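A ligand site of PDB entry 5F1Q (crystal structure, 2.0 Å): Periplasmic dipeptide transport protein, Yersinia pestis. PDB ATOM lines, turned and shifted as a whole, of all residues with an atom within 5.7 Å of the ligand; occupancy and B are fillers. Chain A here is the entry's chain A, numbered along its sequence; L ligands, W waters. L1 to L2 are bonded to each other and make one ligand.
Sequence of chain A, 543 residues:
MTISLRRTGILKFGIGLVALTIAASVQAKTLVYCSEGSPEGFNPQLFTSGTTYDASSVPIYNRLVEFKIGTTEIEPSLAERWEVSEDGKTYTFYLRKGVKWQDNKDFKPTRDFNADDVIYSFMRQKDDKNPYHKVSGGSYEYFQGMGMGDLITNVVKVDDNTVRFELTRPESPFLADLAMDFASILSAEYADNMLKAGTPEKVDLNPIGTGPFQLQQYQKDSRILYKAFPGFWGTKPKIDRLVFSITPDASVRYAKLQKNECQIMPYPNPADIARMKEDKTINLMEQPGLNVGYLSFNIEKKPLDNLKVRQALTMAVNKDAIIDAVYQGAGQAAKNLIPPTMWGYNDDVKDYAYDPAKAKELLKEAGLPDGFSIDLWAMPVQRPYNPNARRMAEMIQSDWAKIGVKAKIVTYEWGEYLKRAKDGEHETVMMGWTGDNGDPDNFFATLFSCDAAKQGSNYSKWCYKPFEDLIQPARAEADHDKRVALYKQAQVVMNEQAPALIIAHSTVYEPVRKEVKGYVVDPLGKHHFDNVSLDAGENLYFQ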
ATOM      1  N   THR A  48      21.559  18.951  14.210  1.00  0.00           N
ATOM      2  CA  THR A  48      20.481  18.744  15.182  1.00  0.00           C
ATOM      3  C   THR A  48      19.131  19.399  14.864  1.00  0.00           C
ATOM      4  O   THR A  48      18.166  19.205  15.601  1.00  0.00           O
ATOM      5  CB  THR A  48      20.909  19.238  16.567  1.00  0.00           C
ATOM      6  OG1 THR A  48      21.082  20.662  16.530  1.00  0.00           O
ATOM      7  CG2 THR A  48      22.208  18.593  16.985  1.00  0.00           C
ATOM      8  N   SER A  49      19.042  20.181  13.790  1.00  0.00           N
ATOM      9  CA  SER A  49      17.800  20.934  13.557  1.00  0.00           C
ATOM     10  C   SER A  49      16.750  20.132  12.763  1.00  0.00           C
ATOM     11  O   SER A  49      17.077  19.333  11.862  1.00  0.00           O
ATOM     12  CB  SER A  49      18.081  22.253  12.826  1.00  0.00           C
ATOM     13  OG  SER A  49      18.181  22.080  11.425  1.00  0.00           O
ATOM     14  N   GLY A  50      15.489  20.333  13.110  1.00  0.00           N
ATOM     15  CA  GLY A  50      14.376  19.748  12.371  1.00  0.00           C
ATOM     16  C   GLY A  50      14.405  20.191  10.907  1.00  0.00           C
ATOM     17  O   GLY A  50      13.994  19.464  10.018  1.00  0.00           O
ATOM     18  N   THR A  51      14.904  21.403  10.671  1.00  0.00           N
ATOM     19  CA  THR A  51      15.029  21.950   9.331  1.00  0.00           C
ATOM     20  C   THR A  51      15.864  20.986   8.476  1.00  0.00           C
ATOM     21  O   THR A  51      15.470  20.578   7.380  1.00  0.00           O
ATOM     22  CB  THR A  51      15.661  23.343   9.388  1.00  0.00           C
ATOM     23  OG1 THR A  51      15.027  24.079  10.433  1.00  0.00           O
ATOM     24  CG2 THR A  51      15.472  24.100   8.054  1.00  0.00           C
ATOM     25  N   TYR A  53      16.656  17.779   9.266  1.00  0.00           N
ATOM     26  CA  TYR A  53      16.128  16.426   9.253  1.00  0.00           C
ATOM     27  C   TYR A  53      15.002  16.273   8.228  1.00  0.00           C
ATOM     28  O   TYR A  53      14.948  15.261   7.517  1.00  0.00           O
ATOM     29  CB  TYR A  53      15.633  16.030  10.650  1.00  0.00           C
ATOM     30  CG  TYR A  53      16.778  15.789  11.639  1.00  0.00           C
ATOM     31  CD1 TYR A  53      18.085  15.639  11.192  1.00  0.00           C
ATOM     32  CD2 TYR A  53      16.529  15.705  13.013  1.00  0.00           C
ATOM     33  CE1 TYR A  53      19.121  15.402  12.090  1.00  0.00           C
ATOM     34  CE2 TYR A  53      17.556  15.479  13.909  1.00  0.00           C
ATOM     35  CZ  TYR A  53      18.843  15.338  13.450  1.00  0.00           C
ATOM     36  OH  TYR A  53      19.859  15.091  14.339  1.00  0.00           O
ATOM     37  N   GLU A 141      26.924  15.567  17.038  1.00  0.00           N
ATOM     38  CA  GLU A 141      26.435  16.246  18.234  1.00  0.00           C
ATOM     39  C   GLU A 141      25.494  15.353  19.068  1.00  0.00           C
ATOM     40  O   GLU A 141      25.692  15.204  20.269  1.00  0.00           O
ATOM     41  CB  GLU A 141      25.729  17.551  17.855  1.00  0.00           C
ATOM     42  CG  GLU A 141      25.334  18.407  19.062  1.00  0.00           C
ATOM     43  CD  GLU A 141      24.877  19.813  18.675  1.00  0.00           C
ATOM     44  OE1 GLU A 141      25.191  20.227  17.539  1.00  0.00           O
ATOM     45  OE2 GLU A 141      24.191  20.482  19.478  1.00  0.00           O
ATOM     46  N   TYR A 142      24.490  14.759  18.442  1.00  0.00           N
ATOM     47  CA  TYR A 142      23.672  13.761  19.131  1.00  0.00           C
ATOM     48  C   TYR A 142      24.467  12.579  19.682  1.00  0.00           C
ATOM     49  O   TYR A 142      24.337  12.219  20.858  1.00  0.00           O
ATOM     50  CB  TYR A 142      22.613  13.202  18.205  1.00  0.00           C
ATOM     51  CG  TYR A 142      21.306  13.932  18.230  1.00  0.00           C
ATOM     52  CD1 TYR A 142      20.352  13.641  19.185  1.00  0.00           C
ATOM     53  CD2 TYR A 142      21.010  14.892  17.268  1.00  0.00           C
ATOM     54  CE1 TYR A 142      19.121  14.311  19.189  1.00  0.00           C
ATOM     55  CE2 TYR A 142      19.799  15.559  17.263  1.00  0.00           C
ATOM     56  CZ  TYR A 142      18.853  15.256  18.210  1.00  0.00           C
ATOM     57  OH  TYR A 142      17.632  15.919  18.184  1.00  0.00           O
ATOM     58  N   ASP A 181      16.983  10.278  14.046  1.00  0.00           N
ATOM     59  CA  ASP A 181      17.602  10.732  12.811  1.00  0.00           C
ATOM     60  C   ASP A 181      19.110  10.520  12.759  1.00  0.00           C
ATOM     61  O   ASP A 181      19.647  10.081  11.736  1.00  0.00           O
ATOM     62  CB  ASP A 181      17.270  12.218  12.593  1.00  0.00           C
ATOM     63  CG  ASP A 181      15.775  12.466  12.568  1.00  0.00           C
ATOM     64  OD1 ASP A 181      15.171  12.568  13.668  1.00  0.00           O
ATOM     65  OD2 ASP A 181      15.199  12.540  11.462  1.00  0.00           O
ATOM     66  N   MET A 379      17.299  33.180  17.399  1.00  0.00           N
ATOM     67  CA  MET A 379      17.387  32.620  16.053  1.00  0.00           C
ATOM     68  C   MET A 379      16.526  33.417  15.060  1.00  0.00           C
ATOM     69  O   MET A 379      15.506  34.009  15.431  1.00  0.00           O
ATOM     70  CB  MET A 379      16.978  31.127  16.052  1.00  0.00           C
ATOM     71  CG  MET A 379      15.518  30.849  16.420  1.00  0.00           C
ATOM     72  SD  MET A 379      15.250  30.594  18.340  1.00  0.00           S
ATOM     73  CE  MET A 379      16.281  28.943  18.573  1.00  0.00           C
ATOM     74  N   ARG A 383      10.625  28.417  14.923  1.00  0.00           N
ATOM     75  CA  ARG A 383      10.803  27.056  15.445  1.00  0.00           C
ATOM     76  C   ARG A 383       9.464  26.543  15.984  1.00  0.00           C
ATOM     77  O   ARG A 383       8.601  27.344  16.339  1.00  0.00           O
ATOM     78  CB  ARG A 383      11.844  27.031  16.581  1.00  0.00           C
ATOM     79  CG  ARG A 383      13.224  27.562  16.222  1.00  0.00           C
ATOM     80  CD  ARG A 383      13.668  27.063  14.864  1.00  0.00           C
ATOM     81  NE  ARG A 383      13.774  25.603  14.765  1.00  0.00           N
ATOM     82  CZ  ARG A 383      13.365  24.878  13.712  1.00  0.00           C
ATOM     83  NH1 ARG A 383      13.583  23.575  13.688  1.00  0.00           N
ATOM     84  NH2 ARG A 383      12.749  25.467  12.683  1.00  0.00           N
ATOM     85  N   PRO A 384       9.288  25.224  16.105  1.00  0.00           N
ATOM     86  CA  PRO A 384       8.012  24.750  16.667  1.00  0.00           C
ATOM     87  C   PRO A 384       7.776  25.235  18.097  1.00  0.00           C
ATOM     88  O   PRO A 384       6.642  25.402  18.490  1.00  0.00           O
ATOM     89  CB  PRO A 384       8.141  23.216  16.620  1.00  0.00           C
ATOM     90  CG  PRO A 384       9.596  22.944  16.427  1.00  0.00           C
ATOM     91  CD  PRO A 384      10.166  24.105  15.681  1.00  0.00           C
ATOM     92  N   TYR A 385       8.835  25.520  18.846  1.00  0.00           N
ATOM     93  CA  TYR A 385       8.717  25.967  20.232  1.00  0.00           C
ATOM     94  C   TYR A 385       8.877  27.493  20.369  1.00  0.00           C
ATOM     95  O   TYR A 385       8.828  28.019  21.477  1.00  0.00           O
ATOM     96  CB  TYR A 385       9.789  25.281  21.083  1.00  0.00           C
ATOM     97  CG  TYR A 385      11.167  25.387  20.440  1.00  0.00           C
ATOM     98  CD1 TYR A 385      11.921  26.555  20.545  1.00  0.00           C
ATOM     99  CD2 TYR A 385      11.691  24.319  19.726  1.00  0.00           C
ATOM    100  CE1 TYR A 385      13.168  26.648  19.946  1.00  0.00           C
ATOM    101  CE2 TYR A 385      12.938  24.411  19.117  1.00  0.00           C
ATOM    102  CZ  TYR A 385      13.671  25.572  19.233  1.00  0.00           C
ATOM    103  OH  TYR A 385      14.917  25.659  18.655  1.00  0.00           O
ATOM    104  N   TRP A 414      20.864  30.567  10.796  1.00  0.00           N
ATOM    105  CA  TRP A 414      20.483  29.401  11.602  1.00  0.00           C
ATOM    106  C   TRP A 414      21.571  28.336  11.838  1.00  0.00           C
ATOM    107  O   TRP A 414      21.843  27.977  12.972  1.00  0.00           O
ATOM    108  CB  TRP A 414      19.253  28.738  10.939  1.00  0.00           C
ATOM    109  CG  TRP A 414      18.553  27.580  11.643  1.00  0.00           C
ATOM    110  CD1 TRP A 414      17.991  26.484  11.029  1.00  0.00           C
ATOM    111  CD2 TRP A 414      18.287  27.422  13.050  1.00  0.00           C
ATOM    112  NE1 TRP A 414      17.405  25.651  11.963  1.00  0.00           N
ATOM    113  CE2 TRP A 414      17.568  26.204  13.208  1.00  0.00           C
ATOM    114  CE3 TRP A 414      18.578  28.181  14.189  1.00  0.00           C
ATOM    115  CZ2 TRP A 414      17.157  25.727  14.466  1.00  0.00           C
ATOM    116  CZ3 TRP A 414      18.167  27.704  15.447  1.00  0.00           C
ATOM    117  CH2 TRP A 414      17.459  26.500  15.572  1.00  0.00           C
ATOM    118  N   LEU A 418      23.613  27.705  15.586  1.00  0.00           N
ATOM    119  CA  LEU A 418      23.769  26.462  16.312  1.00  0.00           C
ATOM    120  C   LEU A 418      25.233  26.088  16.481  1.00  0.00           C
ATOM    121  O   LEU A 418      25.627  25.616  17.552  1.00  0.00           O
ATOM    122  CB  LEU A 418      23.015  25.335  15.603  1.00  0.00           C
ATOM    123  CG  LEU A 418      21.498  25.562  15.622  1.00  0.00           C
ATOM    124  CD1 LEU A 418      20.765  24.567  14.738  1.00  0.00           C
ATOM    125  CD2 LEU A 418      20.986  25.475  17.028  1.00  0.00           C
ATOM    126  N   MET A 431      16.715  28.946  22.657  1.00  0.00           N
ATOM    127  CA  MET A 431      16.908  27.545  22.345  1.00  0.00           C
ATOM    128  C   MET A 431      15.593  26.793  22.568  1.00  0.00           C
ATOM    129  O   MET A 431      14.630  27.362  23.065  1.00  0.00           O
ATOM    130  CB  MET A 431      17.998  26.967  23.239  1.00  0.00           C
ATOM    131  CG  MET A 431      18.978  26.082  22.562  1.00  0.00           C
ATOM    132  SD  MET A 431      20.002  25.104  23.889  1.00  0.00           S
ATOM    133  CE  MET A 431      19.719  23.344  23.091  1.00  0.00           C
ATOM    134  N   GLY A 432      15.555  25.514  22.206  1.00  0.00           N
ATOM    135  CA  GLY A 432      14.357  24.719  22.405  1.00  0.00           C
ATOM    136  C   GLY A 432      14.481  23.307  21.872  1.00  0.00           C
ATOM    137  O   GLY A 432      15.535  22.886  21.391  1.00  0.00           O
ATOM    138  N   TRP A 433      13.387  22.554  21.953  1.00  0.00           N
ATOM    139  CA  TRP A 433      13.460  21.146  21.601  1.00  0.00           C
ATOM    140  C   TRP A 433      12.076  20.615  21.291  1.00  0.00           C
ATOM    141  O   TRP A 433      11.143  20.947  21.969  1.00  0.00           O
ATOM    142  CB  TRP A 433      14.061  20.381  22.782  1.00  0.00           C
ATOM    143  CG  TRP A 433      14.617  19.014  22.544  1.00  0.00           C
ATOM    144  CD1 TRP A 433      14.107  17.825  23.030  1.00  0.00           C
ATOM    145  CD2 TRP A 433      15.832  18.701  21.871  1.00  0.00           C
ATOM    146  NE1 TRP A 433      14.941  16.780  22.665  1.00  0.00           N
ATOM    147  CE2 TRP A 433      16.011  17.298  21.965  1.00  0.00           C
ATOM    148  CE3 TRP A 433      16.802  19.468  21.211  1.00  0.00           C
ATOM    149  CZ2 TRP A 433      17.118  16.638  21.412  1.00  0.00           C
ATOM    150  CZ3 TRP A 433      17.909  18.817  20.657  1.00  0.00           C
ATOM    151  CH2 TRP A 433      18.047  17.408  20.751  1.00  0.00           C
ATOM    152  N   THR A 434      11.971  19.795  20.243  1.00  0.00           N
ATOM    153  CA  THR A 434      10.855  18.864  20.100  1.00  0.00           C
ATOM    154  C   THR A 434      11.456  17.490  20.380  1.00  0.00           C
ATOM    155  O   THR A 434      12.509  17.160  19.833  1.00  0.00           O
ATOM    156  CB  THR A 434      10.231  18.933  18.702  1.00  0.00           C
ATOM    157  OG1 THR A 434       9.747  20.266  18.469  1.00  0.00           O
ATOM    158  CG2 THR A 434       9.068  17.898  18.526  1.00  0.00           C
ATOM    159  N   GLY A 435      10.814  16.702  21.255  1.00  0.00           N
ATOM    160  CA  GLY A 435      11.329  15.389  21.616  1.00  0.00           C
ATOM    161  C   GLY A 435      11.480  14.496  20.377  1.00  0.00           C
ATOM    162  O   GLY A 435      10.683  14.576  19.444  1.00  0.00           O
ATOM    163  N   ASP A 436      12.540  13.687  20.367  1.00  0.00           N
ATOM    164  CA  ASP A 436      12.832  12.813  19.245  1.00  0.00           C
ATOM    165  C   ASP A 436      12.337  11.391  19.385  1.00  0.00           C
ATOM    166  O   ASP A 436      12.240  10.683  18.399  1.00  0.00           O
ATOM    167  CB  ASP A 436      14.346  12.773  19.012  1.00  0.00           C
ATOM    168  CG  ASP A 436      14.930  14.168  18.815  1.00  0.00           C
ATOM    169  OD1 ASP A 436      14.540  14.836  17.822  1.00  0.00           O
ATOM    170  OD2 ASP A 436      15.797  14.569  19.616  1.00  0.00           O
ATOM    171  N   ASN A 442      15.709  11.841  26.434  1.00  0.00           N
ATOM    172  CA  ASN A 442      15.995  12.644  25.243  1.00  0.00           C
ATOM    173  C   ASN A 442      15.831  14.157  25.506  1.00  0.00           C
ATOM    174  O   ASN A 442      16.285  14.982  24.706  1.00  0.00           O
ATOM    175  CB  ASN A 442      15.084  12.157  24.092  1.00  0.00           C
ATOM    176  CG  ASN A 442      15.058  13.086  22.891  1.00  0.00           C
ATOM    177  OD1 ASN A 442      14.049  13.742  22.623  1.00  0.00           O
ATOM    178  ND2 ASN A 442      16.142  13.134  22.128  1.00  0.00           N
ATOM    179  N   SER A 457      24.274  19.263  22.846  1.00  0.00           N
ATOM    180  CA  SER A 457      23.361  20.391  22.762  1.00  0.00           C
ATOM    181  C   SER A 457      23.040  21.052  24.112  1.00  0.00           C
ATOM    182  O   SER A 457      22.029  21.735  24.245  1.00  0.00           O
ATOM    183  CB  SER A 457      22.048  19.946  22.092  1.00  0.00           C
ATOM    184  OG  SER A 457      22.294  19.356  20.821  1.00  0.00           O
ATOM    185  N   TYR A 459      23.712  23.915  25.848  1.00  0.00           N
ATOM    186  CA  TYR A 459      24.358  25.204  25.598  1.00  0.00           C
ATOM    187  C   TYR A 459      24.462  26.034  26.887  1.00  0.00           C
ATOM    188  O   TYR A 459      25.087  27.094  26.899  1.00  0.00           O
ATOM    189  CB  TYR A 459      23.626  25.971  24.488  1.00  0.00           C
ATOM    190  CG  TYR A 459      23.642  25.260  23.117  1.00  0.00           C
ATOM    191  CD1 TYR A 459      24.490  24.157  22.893  1.00  0.00           C
ATOM    192  CD2 TYR A 459      22.832  25.669  22.078  1.00  0.00           C
ATOM    193  CE1 TYR A 459      24.510  23.503  21.675  1.00  0.00           C
ATOM    194  CE2 TYR A 459      22.841  25.014  20.850  1.00  0.00           C
ATOM    195  CZ  TYR A 459      23.681  23.934  20.643  1.00  0.00           C
ATOM    196  OH  TYR A 459      23.679  23.270  19.416  1.00  0.00           O
ATOM    197  N   LEU A 524       6.747  14.130  17.092  1.00  0.00           N
ATOM    198  CA  LEU A 524       8.204  14.297  17.149  1.00  0.00           C
ATOM    199  C   LEU A 524       8.711  15.398  16.200  1.00  0.00           C
ATOM    200  O   LEU A 524       9.923  15.617  16.088  1.00  0.00           O
ATOM    201  CB  LEU A 524       8.882  12.950  16.845  1.00  0.00           C
ATOM    202  CG  LEU A 524       8.290  11.766  17.625  1.00  0.00           C
ATOM    203  CD1 LEU A 524       9.024  10.476  17.261  1.00  0.00           C
ATOM    204  CD2 LEU A 524       8.356  12.006  19.136  1.00  0.00           C
ATOM    205  N   GLY A 525       7.800  16.114  15.546  1.00  0.00           N
ATOM    206  CA  GLY A 525       8.138  17.396  14.923  1.00  0.00           C
ATOM    207  C   GLY A 525       8.662  17.387  13.493  1.00  0.00           C
ATOM    208  O   GLY A 525       8.981  18.436  12.929  1.00  0.00           O
ATOM    209  N   LYS A 526       8.786  16.225  12.877  1.00  0.00           N
ATOM    210  CA  LYS A 526       9.230  16.221  11.496  1.00  0.00           C
ATOM    211  C   LYS A 526       8.016  16.243  10.565  1.00  0.00           C
ATOM    212  O   LYS A 526       6.891  16.018  10.983  1.00  0.00           O
ATOM    213  CB  LYS A 526      10.141  15.021  11.208  1.00  0.00           C
ATOM    214  CG  LYS A 526      11.600  15.364  11.468  1.00  0.00           C
ATOM    215  CD  LYS A 526      12.377  14.218  12.043  1.00  0.00           C
ATOM    216  CE  LYS A 526      11.693  13.697  13.270  1.00  0.00           C
ATOM    217  NZ  LYS A 526      12.565  12.768  14.031  1.00  0.00           N
HETATM  218  N1  LIG L   1      15.011  17.456  18.565  1.00  0.00           N
HETATM  219  C1  LIG L   1      15.699  18.296  17.600  1.00  0.00           C
HETATM  220  C2  LIG L   1      15.470  19.758  17.892  1.00  0.00           C
HETATM  221  O1  LIG L   1      14.461  20.133  18.492  1.00  0.00           O
HETATM  222  C3  LIG L   1      15.215  17.984  16.184  1.00  0.00           C
HETATM  223  C4  LIG L   1      13.801  17.473  16.154  1.00  0.00           C
HETATM  224  C5  LIG L   1      12.874  18.356  15.401  1.00  0.00           C
HETATM  225  O2  LIG L   1      11.900  17.887  14.805  1.00  0.00           O
HETATM  226  N2  LIG L   1      13.149  19.669  15.412  1.00  0.00           N
HETATM  227  N1  LG2 L   2      16.374  20.601  17.412  1.00  0.00           N
HETATM  228  C1  LG2 L   2      16.315  22.039  17.646  1.00  0.00           C
HETATM  229  C2  LG2 L   2      15.579  22.750  16.505  1.00  0.00           C
HETATM  230  O1  LG2 L   2      15.178  23.913  16.636  1.00  0.00           O
HETATM  231  C3  LG2 L   2      17.752  22.593  17.821  1.00  0.00           C
HETATM  232  C4  LG2 L   2      18.396  22.147  19.161  1.00  0.00           C
HETATM  233  C5  LG2 L   2      19.927  22.351  19.232  1.00  0.00           C
HETATM  234  O2  LG2 L   2      20.718  21.519  18.780  1.00  0.00           O
HETATM  235  N2  LG2 L   2      20.340  23.462  19.803  1.00  0.00           N
HETATM  236  O3  LG2 L   2      15.351  22.151  15.441  1.00  0.00           O
HETATM  237  O   HOH W   1      12.406  14.293  16.178  1.00  0.00           O
HETATM  238  O   HOH W   2      12.154  21.426  17.574  1.00  0.00           O
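The backbone carbonyl oxygen of Thr 48 is in hydrogen-bond range of a nitrogen (N1) of LG2 L2 (2.9 Å). O2 of LG2 L2 sits at hydrogen-bond distance from OG1 of Thr 48 (2.4 Å). The side-chain hydroxyl of Tyr 385 is in hydrogen-bond range of an oxygen (O1) of LG2 L2, 2.7 Å away. OD1 of Asp 436 lies within salt-bridge range of N1 of LIG L1 (2.8 Å). N of Thr 434 is in hydrogen-bond range of O1 of LIG L1, 3.1 Å away. O of Thr 434 sits at hydrogen-bond distance from N1 of LIG L1, 2.8 Å away. NH1 of Arg 383 lies within salt-bridge range of O3 of LG2 L2, 2.9 Å away. The backbone NH (N) of Gly 50 is in hydrogen-bond range of an oxygen (O3) of LG2 L2 (3.0 Å). A nitrogen (N1) of LIG L1 sits at hydrogen-bond distance from the side-chain hydroxyl of Tyr 142 (3.1 Å). The side-chain hydroxyl (OH) of Tyr 459 sits close to a nitrogen (N2) of LG2 L2 (3.4 Å). OG of Ser 457 sits at hydrogen-bond distance from O2 of LG2 L2, 3.4 Å away.
The side-chain carboxylate (OD2) of Asp 436 is in hydrogen-bond range of the side-chain hydroxyl (OH) of Tyr 142, 2.7 Å away. The side-chain amide oxygen (OD1) of Asn 442 lies within hydrogen-bond range of the backbone NH (N) of Asp 436 (2.7 Å). The guanidinium group (NH2) of Arg 383 lies within hydrogen-bond range of the side-chain hydroxyl (OG1) of Thr 51, at 3.5 Å. The side-chain hydroxyl of Tyr 459 lies within hydrogen-bond range of the side-chain carboxylate of Glu 141 (2.8 Å). The side-chain hydroxyl of Ser 49 sits close to the backbone NH of Thr 51 (3.4 Å). The side-chain hydroxyl of Ser 457 lies within hydrogen-bond range of the side-chain carboxylate of Glu 141 (2.6 Å). NE1 of Trp 433 lies within hydrogen-bond range of O of Asn 442 (3.0 Å). The indole nitrogen (NE1) of Trp 414 lies within hydrogen-bond range of the side-chain hydroxyl (OG1) of Thr 51, 3.2 Å away.
An oxygen (O2) of LIG L1 lies close to the backbone carbonyl oxygen (O) of Leu 524 (3.3 Å). Residues that only touch the ligand: Ser 49, Glu 141, Trp 414, Leu 418, Met 431, Gly 432, Trp 433 and Gly 525. Hydrophobic or aromatic side chains that line the ligand: Tyr 385, Trp 414, Leu 418, Met 431, Trp 433 and Tyr 459. Within 4 Å of the ligand: Thr 48, Ser 49, Gly 50, Glu 141, Tyr 142, Arg 383, Tyr 385, Trp 414, Leu 418, Met 431, Gly 432, Trp 433, Thr 434, Asp 436, Ser 457, Tyr 459, Leu 524 and Gly 525.
Water W2 bridges an oxygen (O1) of LIG L1 (2.8 Å) and the side-chain hydroxyl of Thr 434 (2.8 Å). Water W1 lies within hydrogen-bond range of the side-chain amino group of Lys 526 (2.6 Å), the side-chain carboxylate of Asp 436 (2.7 Å) and the backbone carbonyl oxygen of Leu 524 (2.8 Å).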
